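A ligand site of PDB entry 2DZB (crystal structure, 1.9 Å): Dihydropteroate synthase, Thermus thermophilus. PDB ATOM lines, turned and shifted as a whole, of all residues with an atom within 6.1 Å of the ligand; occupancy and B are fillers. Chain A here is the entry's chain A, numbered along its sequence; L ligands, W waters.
The guanidinium group (NH1) of Arg 268 lies within salt-bridge range of an oxygen (O6) of the ligand (2.8 Å). The side-chain amide oxygen (OD1) of Asn 128 sits at hydrogen-bond distance from a nitrogen (N4) of the ligand, at 2.7 Å. An oxygen (O6) of the ligand is in hydrogen-bond range of a ring nitrogen (NE2) of His 270 (2.5 Å). N5 of the ligand sits at hydrogen-bond distance from SD of Met 152 (3.4 Å). The side-chain carboxylate of Asp 197 is in hydrogen-bond range of a nitrogen (N5) of the ligand, at 2.6 Å. The side-chain amide nitrogen of Asn 36 lies within hydrogen-bond range of an oxygen (O8) of the ligand, at 3.4 Å. NZ of Lys 233 is in hydrogen-bond range of O1 of the ligand (3.0 Å). OD2 of Asp 109 sits at hydrogen-bond distance from N2 of the ligand (2.8 Å).
The backbone carbonyl oxygen of Gly 229 sits close to an oxygen (O1) of the ligand (3.5 Å). CG1 of Val 34 touches O6 of the ligand (3.5 Å). Val 130 touches the ligand. CG1 of Val 150 touches N4 of the ligand (3.7 Å). CE1 of Phe 202 touches N1 of the ligand (3.3 Å). Leu 227 touches the ligand. Within 4 Å of the ligand: Val 34, Asn 36, Asp 109, Asn 128, Val 130, Val 150, Met 152, Asp 197, Phe 202, Leu 227, Gly 229, Lys 233, Arg 268 and His 270. The nearest printed residue that does not touch the ligand is Glu 74 (4.01 Å).
OD2 of Asp 109 lies within salt-bridge range of NH2 of Arg 268 (3.5 Å). The backbone carbonyl oxygen of Val 150 lies within hydrogen-bond range of the backbone NH of Asp 129 (3.4 Å). The guanidinium group of Arg 268 is in salt-bridge range of the side-chain carboxylate of Asp 70 (2.9 Å). ND2 of Asn 128 sits at hydrogen-bond distance from OD2 of Asp 109. The side-chain amino group of Lys 233 is in hydrogen-bond range of the backbone carbonyl oxygen of Gly 229 (2.7 Å). The backbone carbonyl oxygen (O) of Phe 200 sits at hydrogen-bond distance from the side-chain amino group (NZ) of Lys 233 (2.8 Å). OD1 of Asp 197 lies within hydrogen-bond range of N of Gly 199. N of Arg 268 lies within hydrogen-bond range of O of Val 228.
Water W3 lies within hydrogen-bond range of OE2 of Glu 74 (2.4 Å) and O7 of the ligand (2.7 Å). Water W5 lies within hydrogen-bond range of the side-chain carboxylate of Asp 197 (2.5 Å), an oxygen (O1) of the ligand (3.0 Å), the backbone NH of Phe 200 (3.0 Å) and the backbone NH of Gly 229 (3.1 Å). Water W1 bridges an oxygen (O7) of the ligand (3.1 Å) and the side-chain amide oxygen (OD1) of Asn 36 (3.4 Å). Water W2 lies within hydrogen-bond range of O of Ser 231 (2.6 Å) and O2 of the ligand (3.3 Å).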
ATOM      1  N   VAL A  34      23.268  15.622 -16.253  1.00  0.00           N
ATOM      2  CA  VAL A  34      23.993  16.855 -15.941  1.00  0.00           C
ATOM      3  C   VAL A  34      23.944  17.280 -14.478  1.00  0.00           C
ATOM      4  O   VAL A  34      22.896  17.287 -13.842  1.00  0.00           O
ATOM      5  CB  VAL A  34      23.469  18.033 -16.791  1.00  0.00           C
ATOM      6  CG1 VAL A  34      24.171  19.327 -16.401  1.00  0.00           C
ATOM      7  CG2 VAL A  34      23.694  17.742 -18.268  1.00  0.00           C
ATOM      8  N   ASN A  36      25.311  20.509 -12.788  1.00  0.00           N
ATOM      9  CA  ASN A  36      25.920  21.832 -12.959  1.00  0.00           C
ATOM     10  C   ASN A  36      26.291  22.466 -11.625  1.00  0.00           C
ATOM     11  O   ASN A  36      25.449  22.651 -10.752  1.00  0.00           O
ATOM     12  CB  ASN A  36      24.948  22.735 -13.726  1.00  0.00           C
ATOM     13  CG  ASN A  36      25.540  24.094 -14.052  1.00  0.00           C
ATOM     14  OD1 ASN A  36      26.763  24.280 -13.997  1.00  0.00           O
ATOM     15  ND2 ASN A  36      24.692  25.049 -14.407  1.00  0.00           N
ATOM     16  N   ASP A  70      27.671  13.824 -15.724  1.00  0.00           N
ATOM     17  CA  ASP A  70      28.445  14.908 -16.331  1.00  0.00           C
ATOM     18  C   ASP A  70      28.517  16.108 -15.376  1.00  0.00           C
ATOM     19  O   ASP A  70      27.526  16.781 -15.129  1.00  0.00           O
ATOM     20  CB  ASP A  70      27.780  15.320 -17.653  1.00  0.00           C
ATOM     21  CG  ASP A  70      28.626  16.288 -18.466  1.00  0.00           C
ATOM     22  OD1 ASP A  70      29.811  15.989 -18.717  1.00  0.00           O
ATOM     23  OD2 ASP A  70      28.095  17.347 -18.861  1.00  0.00           O
ATOM     24  N   GLU A  74      32.130  24.922 -15.338  1.00  0.00           N
ATOM     25  CA  GLU A  74      32.315  25.944 -16.380  1.00  0.00           C
ATOM     26  C   GLU A  74      31.036  26.780 -16.553  1.00  0.00           C
ATOM     27  O   GLU A  74      29.976  26.450 -16.050  1.00  0.00           O
ATOM     28  CB  GLU A  74      32.630  25.217 -17.684  1.00  0.00           C
ATOM     29  CG  GLU A  74      31.817  23.919 -17.846  1.00  0.00           C
ATOM     30  CD  GLU A  74      30.982  23.996 -19.096  1.00  0.00           C
ATOM     31  OE1 GLU A  74      31.548  24.138 -20.167  1.00  0.00           O
ATOM     32  OE2 GLU A  74      29.758  23.903 -18.991  1.00  0.00           O
ATOM     33  N   SER A  75      31.186  27.913 -17.267  1.00  0.00           N
ATOM     34  CA  SER A  75      29.993  28.709 -17.566  1.00  0.00           C
ATOM     35  C   SER A  75      29.752  28.816 -19.075  1.00  0.00           C
ATOM     36  O   SER A  75      28.731  28.389 -19.600  1.00  0.00           O
ATOM     37  CB  SER A  75      30.186  30.109 -16.974  1.00  0.00           C
ATOM     38  OG  SER A  75      29.762  30.102 -15.611  1.00  0.00           O
ATOM     39  N   ASP A 109      33.028  18.257 -17.597  1.00  0.00           N
ATOM     40  CA  ASP A 109      32.784  19.299 -18.580  1.00  0.00           C
ATOM     41  C   ASP A 109      33.682  20.488 -18.261  1.00  0.00           C
ATOM     42  O   ASP A 109      33.342  21.304 -17.409  1.00  0.00           O
ATOM     43  CB  ASP A 109      31.320  19.734 -18.525  1.00  0.00           C
ATOM     44  CG  ASP A 109      30.904  20.541 -19.748  1.00  0.00           C
ATOM     45  OD1 ASP A 109      31.709  21.364 -20.232  1.00  0.00           O
ATOM     46  OD2 ASP A 109      29.758  20.364 -20.214  1.00  0.00           O
ATOM     47  N   ASN A 128      34.835  16.084 -21.435  1.00  0.00           N
ATOM     48  CA  ASN A 128      33.873  16.769 -22.284  1.00  0.00           C
ATOM     49  C   ASN A 128      34.384  18.187 -22.536  1.00  0.00           C
ATOM     50  O   ASN A 128      34.285  19.054 -21.667  1.00  0.00           O
ATOM     51  CB  ASN A 128      32.503  16.794 -21.588  1.00  0.00           C
ATOM     52  CG  ASN A 128      31.441  17.493 -22.412  1.00  0.00           C
ATOM     53  OD1 ASN A 128      31.517  17.550 -23.647  1.00  0.00           O
ATOM     54  ND2 ASN A 128      30.427  18.026 -21.734  1.00  0.00           N
ATOM     55  N   ASP A 129      34.937  18.407 -23.731  1.00  0.00           N
ATOM     56  CA  ASP A 129      35.508  19.693 -24.114  1.00  0.00           C
ATOM     57  C   ASP A 129      34.643  20.472 -25.110  1.00  0.00           C
ATOM     58  O   ASP A 129      34.632  20.163 -26.306  1.00  0.00           O
ATOM     59  CB  ASP A 129      36.901  19.451 -24.717  1.00  0.00           C
ATOM     60  CG  ASP A 129      37.607  20.730 -25.127  1.00  0.00           C
ATOM     61  OD1 ASP A 129      37.163  21.834 -24.749  1.00  0.00           O
ATOM     62  OD2 ASP A 129      38.637  20.618 -25.823  1.00  0.00           O
ATOM     63  N   VAL A 130      33.947  21.494 -24.624  1.00  0.00           N
ATOM     64  CA  VAL A 130      33.093  22.291 -25.493  1.00  0.00           C
ATOM     65  C   VAL A 130      33.896  23.010 -26.583  1.00  0.00           C
ATOM     66  O   VAL A 130      33.364  23.333 -27.639  1.00  0.00           O
ATOM     67  CB  VAL A 130      32.253  23.350 -24.700  1.00  0.00           C
ATOM     68  CG1 VAL A 130      31.327  22.638 -23.709  1.00  0.00           C
ATOM     69  CG2 VAL A 130      33.163  24.341 -23.982  1.00  0.00           C
ATOM     70  N   VAL A 150      35.082  14.066 -25.691  1.00  0.00           N
ATOM     71  CA  VAL A 150      33.980  14.526 -26.518  1.00  0.00           C
ATOM     72  C   VAL A 150      34.454  15.765 -27.278  1.00  0.00           C
ATOM     73  O   VAL A 150      34.921  16.717 -26.659  1.00  0.00           O
ATOM     74  CB  VAL A 150      32.753  14.961 -25.675  1.00  0.00           C
ATOM     75  CG1 VAL A 150      31.660  15.508 -26.599  1.00  0.00           C
ATOM     76  CG2 VAL A 150      32.221  13.784 -24.861  1.00  0.00           C
ATOM     77  N   MET A 152      33.125  18.666 -29.182  1.00  0.00           N
ATOM     78  CA  MET A 152      31.887  19.394 -29.486  1.00  0.00           C
ATOM     79  C   MET A 152      32.221  20.550 -30.415  1.00  0.00           C
ATOM     80  O   MET A 152      33.359  21.042 -30.413  1.00  0.00           O
ATOM     81  CB  MET A 152      31.255  19.934 -28.208  1.00  0.00           C
ATOM     82  CG  MET A 152      29.815  20.420 -28.396  1.00  0.00           C
ATOM     83  SD  MET A 152      29.182  21.357 -27.003  1.00  0.00           S
ATOM     84  CE  MET A 152      29.723  23.027 -27.496  1.00  0.00           C
ATOM     85  N   ASP A 197      29.951  15.726 -31.101  1.00  0.00           N
ATOM     86  CA  ASP A 197      28.766  16.451 -30.665  1.00  0.00           C
ATOM     87  C   ASP A 197      28.692  17.746 -31.486  1.00  0.00           C
ATOM     88  O   ASP A 197      29.593  18.563 -31.415  1.00  0.00           O
ATOM     89  CB  ASP A 197      28.897  16.792 -29.177  1.00  0.00           C
ATOM     90  CG  ASP A 197      27.643  17.419 -28.593  1.00  0.00           C
ATOM     91  OD1 ASP A 197      26.903  18.093 -29.336  1.00  0.00           O
ATOM     92  OD2 ASP A 197      27.409  17.241 -27.384  1.00  0.00           O
ATOM     93  N   GLY A 199      27.200  20.316 -30.996  1.00  0.00           N
ATOM     94  CA  GLY A 199      27.064  21.480 -30.141  1.00  0.00           C
ATOM     95  C   GLY A 199      25.834  22.343 -30.375  1.00  0.00           C
ATOM     96  O   GLY A 199      25.953  23.507 -30.773  1.00  0.00           O
ATOM     97  N   PHE A 200      24.648  21.790 -30.133  1.00  0.00           N
ATOM     98  CA  PHE A 200      23.438  22.588 -30.342  1.00  0.00           C
ATOM     99  C   PHE A 200      23.407  23.814 -29.426  1.00  0.00           C
ATOM    100  O   PHE A 200      23.731  23.736 -28.237  1.00  0.00           O
ATOM    101  CB  PHE A 200      22.187  21.709 -30.121  1.00  0.00           C
ATOM    102  CG  PHE A 200      21.967  20.698 -31.196  1.00  0.00           C
ATOM    103  CD1 PHE A 200      21.504  21.085 -32.456  1.00  0.00           C
ATOM    104  CD2 PHE A 200      22.245  19.347 -30.977  1.00  0.00           C
ATOM    105  CE1 PHE A 200      21.336  20.157 -33.482  1.00  0.00           C
ATOM    106  CE2 PHE A 200      22.076  18.405 -31.993  1.00  0.00           C
ATOM    107  CZ  PHE A 200      21.619  18.798 -33.243  1.00  0.00           C
ATOM    108  N   PHE A 202      25.324  26.479 -29.668  1.00  0.00           N
ATOM    109  CA  PHE A 202      26.621  27.121 -29.569  1.00  0.00           C
ATOM    110  C   PHE A 202      26.975  27.770 -30.912  1.00  0.00           C
ATOM    111  O   PHE A 202      27.353  27.092 -31.863  1.00  0.00           O
ATOM    112  CB  PHE A 202      27.717  26.108 -29.197  1.00  0.00           C
ATOM    113  CG  PHE A 202      27.666  25.667 -27.762  1.00  0.00           C
ATOM    114  CD1 PHE A 202      26.791  24.675 -27.350  1.00  0.00           C
ATOM    115  CD2 PHE A 202      28.479  26.279 -26.816  1.00  0.00           C
ATOM    116  CE1 PHE A 202      26.732  24.300 -26.006  1.00  0.00           C
ATOM    117  CE2 PHE A 202      28.428  25.914 -25.475  1.00  0.00           C
ATOM    118  CZ  PHE A 202      27.553  24.913 -25.067  1.00  0.00           C
ATOM    119  N   LEU A 227      26.991  12.318 -29.558  1.00  0.00           N
ATOM    120  CA  LEU A 227      26.332  12.801 -28.354  1.00  0.00           C
ATOM    121  C   LEU A 227      25.641  14.123 -28.681  1.00  0.00           C
ATOM    122  O   LEU A 227      26.207  14.962 -29.369  1.00  0.00           O
ATOM    123  CB  LEU A 227      27.370  13.057 -27.264  1.00  0.00           C
ATOM    124  CG  LEU A 227      26.937  13.929 -26.086  1.00  0.00           C
ATOM    125  CD1 LEU A 227      25.998  13.145 -25.188  1.00  0.00           C
ATOM    126  CD2 LEU A 227      28.145  14.399 -25.296  1.00  0.00           C
ATOM    127  N   VAL A 228      24.408  14.289 -28.218  1.00  0.00           N
ATOM    128  CA  VAL A 228      23.728  15.573 -28.444  1.00  0.00           C
ATOM    129  C   VAL A 228      23.153  16.024 -27.117  1.00  0.00           C
ATOM    130  O   VAL A 228      22.961  15.227 -26.193  1.00  0.00           O
ATOM    131  CB  VAL A 228      22.579  15.502 -29.504  1.00  0.00           C
ATOM    132  CG1 VAL A 228      23.109  14.983 -30.836  1.00  0.00           C
ATOM    133  CG2 VAL A 228      21.415  14.670 -28.996  1.00  0.00           C
ATOM    134  N   GLY A 229      22.890  17.323 -27.015  1.00  0.00           N
ATOM    135  CA  GLY A 229      22.330  17.853 -25.794  1.00  0.00           C
ATOM    136  C   GLY A 229      21.400  18.993 -26.130  1.00  0.00           C
ATOM    137  O   GLY A 229      21.849  20.093 -26.430  1.00  0.00           O
ATOM    138  N   LEU A 230      20.098  18.725 -26.108  1.00  0.00           N
ATOM    139  CA  LEU A 230      19.116  19.756 -26.419  1.00  0.00           C
ATOM    140  C   LEU A 230      18.319  20.164 -25.194  1.00  0.00           C
ATOM    141  O   LEU A 230      17.544  21.119 -25.242  1.00  0.00           O
ATOM    142  CB  LEU A 230      18.205  19.260 -27.536  1.00  0.00           C
ATOM    143  CG  LEU A 230      18.987  19.285 -28.861  1.00  0.00           C
ATOM    144  CD1 LEU A 230      18.675  18.086 -29.708  1.00  0.00           C
ATOM    145  CD2 LEU A 230      18.688  20.575 -29.591  1.00  0.00           C
ATOM    146  N   SER A 231      18.523  19.453 -24.077  1.00  0.00           N
ATOM    147  CA  SER A 231      17.825  19.757 -22.834  1.00  0.00           C
ATOM    148  C   SER A 231      17.931  21.233 -22.457  1.00  0.00           C
ATOM    149  O   SER A 231      18.999  21.813 -22.378  1.00  0.00           O
ATOM    150  CB  SER A 231      18.459  18.899 -21.721  1.00  0.00           C
ATOM    151  OG  SER A 231      18.023  17.545 -21.853  1.00  0.00           O
ATOM    152  N   ARG A 232      16.750  21.855 -22.274  1.00  0.00           N
ATOM    153  CA  ARG A 232      16.728  23.219 -21.775  1.00  0.00           C
ATOM    154  C   ARG A 232      17.152  24.258 -22.827  1.00  0.00           C
ATOM    155  O   ARG A 232      17.180  25.441 -22.558  1.00  0.00           O
ATOM    156  CB  ARG A 232      17.654  23.278 -20.545  1.00  0.00           C
ATOM    157  CG  ARG A 232      17.017  22.674 -19.294  1.00  0.00           C
ATOM    158  CD  ARG A 232      17.719  23.146 -18.009  1.00  0.00           C
ATOM    159  NE  ARG A 232      17.384  24.552 -17.734  1.00  0.00           N
ATOM    160  CZ  ARG A 232      18.349  25.310 -17.189  1.00  0.00           C
ATOM    161  NH1 ARG A 232      19.539  24.796 -16.929  1.00  0.00           N
ATOM    162  NH2 ARG A 232      18.106  26.602 -16.923  1.00  0.00           N
ATOM    163  N   LYS A 233      17.513  23.796 -24.050  1.00  0.00           N
ATOM    164  CA  LYS A 233      18.096  24.711 -25.048  1.00  0.00           C
ATOM    165  C   LYS A 233      17.074  25.653 -25.694  1.00  0.00           C
ATOM    166  O   LYS A 233      15.864  25.415 -25.728  1.00  0.00           O
ATOM    167  CB  LYS A 233      18.777  23.860 -26.128  1.00  0.00           C
ATOM    168  CG  LYS A 233      19.993  23.105 -25.588  1.00  0.00           C
ATOM    169  CD  LYS A 233      21.225  24.003 -25.467  1.00  0.00           C
ATOM    170  CE  LYS A 233      22.413  23.284 -24.811  1.00  0.00           C
ATOM    171  NZ  LYS A 233      23.091  22.443 -25.799  1.00  0.00           N
ATOM    172  N   ARG A 268      22.856  14.091 -23.569  1.00  0.00           N
ATOM    173  CA  ARG A 268      23.229  14.891 -22.403  1.00  0.00           C
ATOM    174  C   ARG A 268      21.904  15.485 -21.942  1.00  0.00           C
ATOM    175  O   ARG A 268      21.335  16.338 -22.615  1.00  0.00           O
ATOM    176  CB  ARG A 268      24.212  15.999 -22.817  1.00  0.00           C
ATOM    177  CG  ARG A 268      24.760  16.782 -21.633  1.00  0.00           C
ATOM    178  CD  ARG A 268      25.865  17.736 -22.045  1.00  0.00           C
ATOM    179  NE  ARG A 268      26.399  18.457 -20.891  1.00  0.00           N
ATOM    180  CZ  ARG A 268      25.829  19.531 -20.354  1.00  0.00           C
ATOM    181  NH1 ARG A 268      24.710  20.019 -20.865  1.00  0.00           N
ATOM    182  NH2 ARG A 268      26.384  20.114 -19.299  1.00  0.00           N
ATOM    183  N   HIS A 270      19.023  16.763 -18.556  1.00  0.00           N
ATOM    184  CA  HIS A 270      18.827  17.276 -17.203  1.00  0.00           C
ATOM    185  C   HIS A 270      17.806  16.416 -16.451  1.00  0.00           C
ATOM    186  O   HIS A 270      18.034  16.047 -15.312  1.00  0.00           O
ATOM    187  CB  HIS A 270      18.363  18.736 -17.244  1.00  0.00           C
ATOM    188  CG  HIS A 270      19.494  19.707 -17.384  1.00  0.00           C
ATOM    189  ND1 HIS A 270      20.199  20.191 -16.312  1.00  0.00           N
ATOM    190  CD2 HIS A 270      20.084  20.222 -18.489  1.00  0.00           C
ATOM    191  CE1 HIS A 270      21.181  20.971 -16.734  1.00  0.00           C
ATOM    192  NE2 HIS A 270      21.137  21.009 -18.054  1.00  0.00           N
HETATM  193  N1  LIG L   1      25.696  22.023 -23.793  1.00  0.00           N
HETATM  194  C1  LIG L   1      25.917  22.810 -22.780  1.00  0.00           C
HETATM  195  C2  LIG L   1      27.133  22.675 -21.763  1.00  0.00           C
HETATM  196  N2  LIG L   1      28.018  21.503 -22.133  1.00  0.00           N
HETATM  197  N3  LIG L   1      28.611  19.575 -23.578  1.00  0.00           N
HETATM  198  C3  LIG L   1      28.337  18.790 -24.670  1.00  0.00           C
HETATM  199  N4  LIG L   1      29.146  17.745 -25.010  1.00  0.00           N
HETATM  200  N5  LIG L   1      27.172  19.042 -25.492  1.00  0.00           N
HETATM  201  C4  LIG L   1      26.251  20.133 -25.214  1.00  0.00           C
HETATM  202  O1  LIG L   1      25.285  20.384 -25.861  1.00  0.00           O
HETATM  203  C5  LIG L   1      26.563  20.958 -24.067  1.00  0.00           C
HETATM  204  C6  LIG L   1      27.759  20.662 -23.250  1.00  0.00           C
HETATM  205  C7  LIG L   1      24.937  23.893 -22.638  1.00  0.00           C
HETATM  206  O2  LIG L   1      24.106  23.575 -21.464  1.00  0.00           O
HETATM  207  P1  LIG L   1      23.614  24.690 -20.620  1.00  0.00           P
HETATM  208  O3  LIG L   1      22.556  25.667 -21.145  1.00  0.00           O
HETATM  209  O4  LIG L   1      24.777  25.571 -20.128  1.00  0.00           O
HETATM  210  O5  LIG L   1      23.065  24.018 -19.296  1.00  0.00           O
HETATM  211  P2  LIG L   1      23.833  22.909 -18.423  1.00  0.00           P
HETATM  212  O6  LIG L   1      23.434  21.579 -18.993  1.00  0.00           O
HETATM  213  O7  LIG L   1      25.320  23.032 -18.553  1.00  0.00           O
HETATM  214  O8  LIG L   1      23.468  23.065 -16.938  1.00  0.00           O
HETATM  215  O   HOH W   1      27.404  22.050 -16.503  1.00  0.00           O
HETATM  216  O   HOH W   2      21.585  21.454 -22.035  1.00  0.00           O
HETATM  217  O   HOH W   3      27.466  24.603 -18.800  1.00  0.00           O
HETATM  218  O   HOH W   4      23.557  26.848 -23.867  1.00  0.00           O
HETATM  219  O   HOH W   5      24.821  19.259 -28.574  1.00  0.00           O
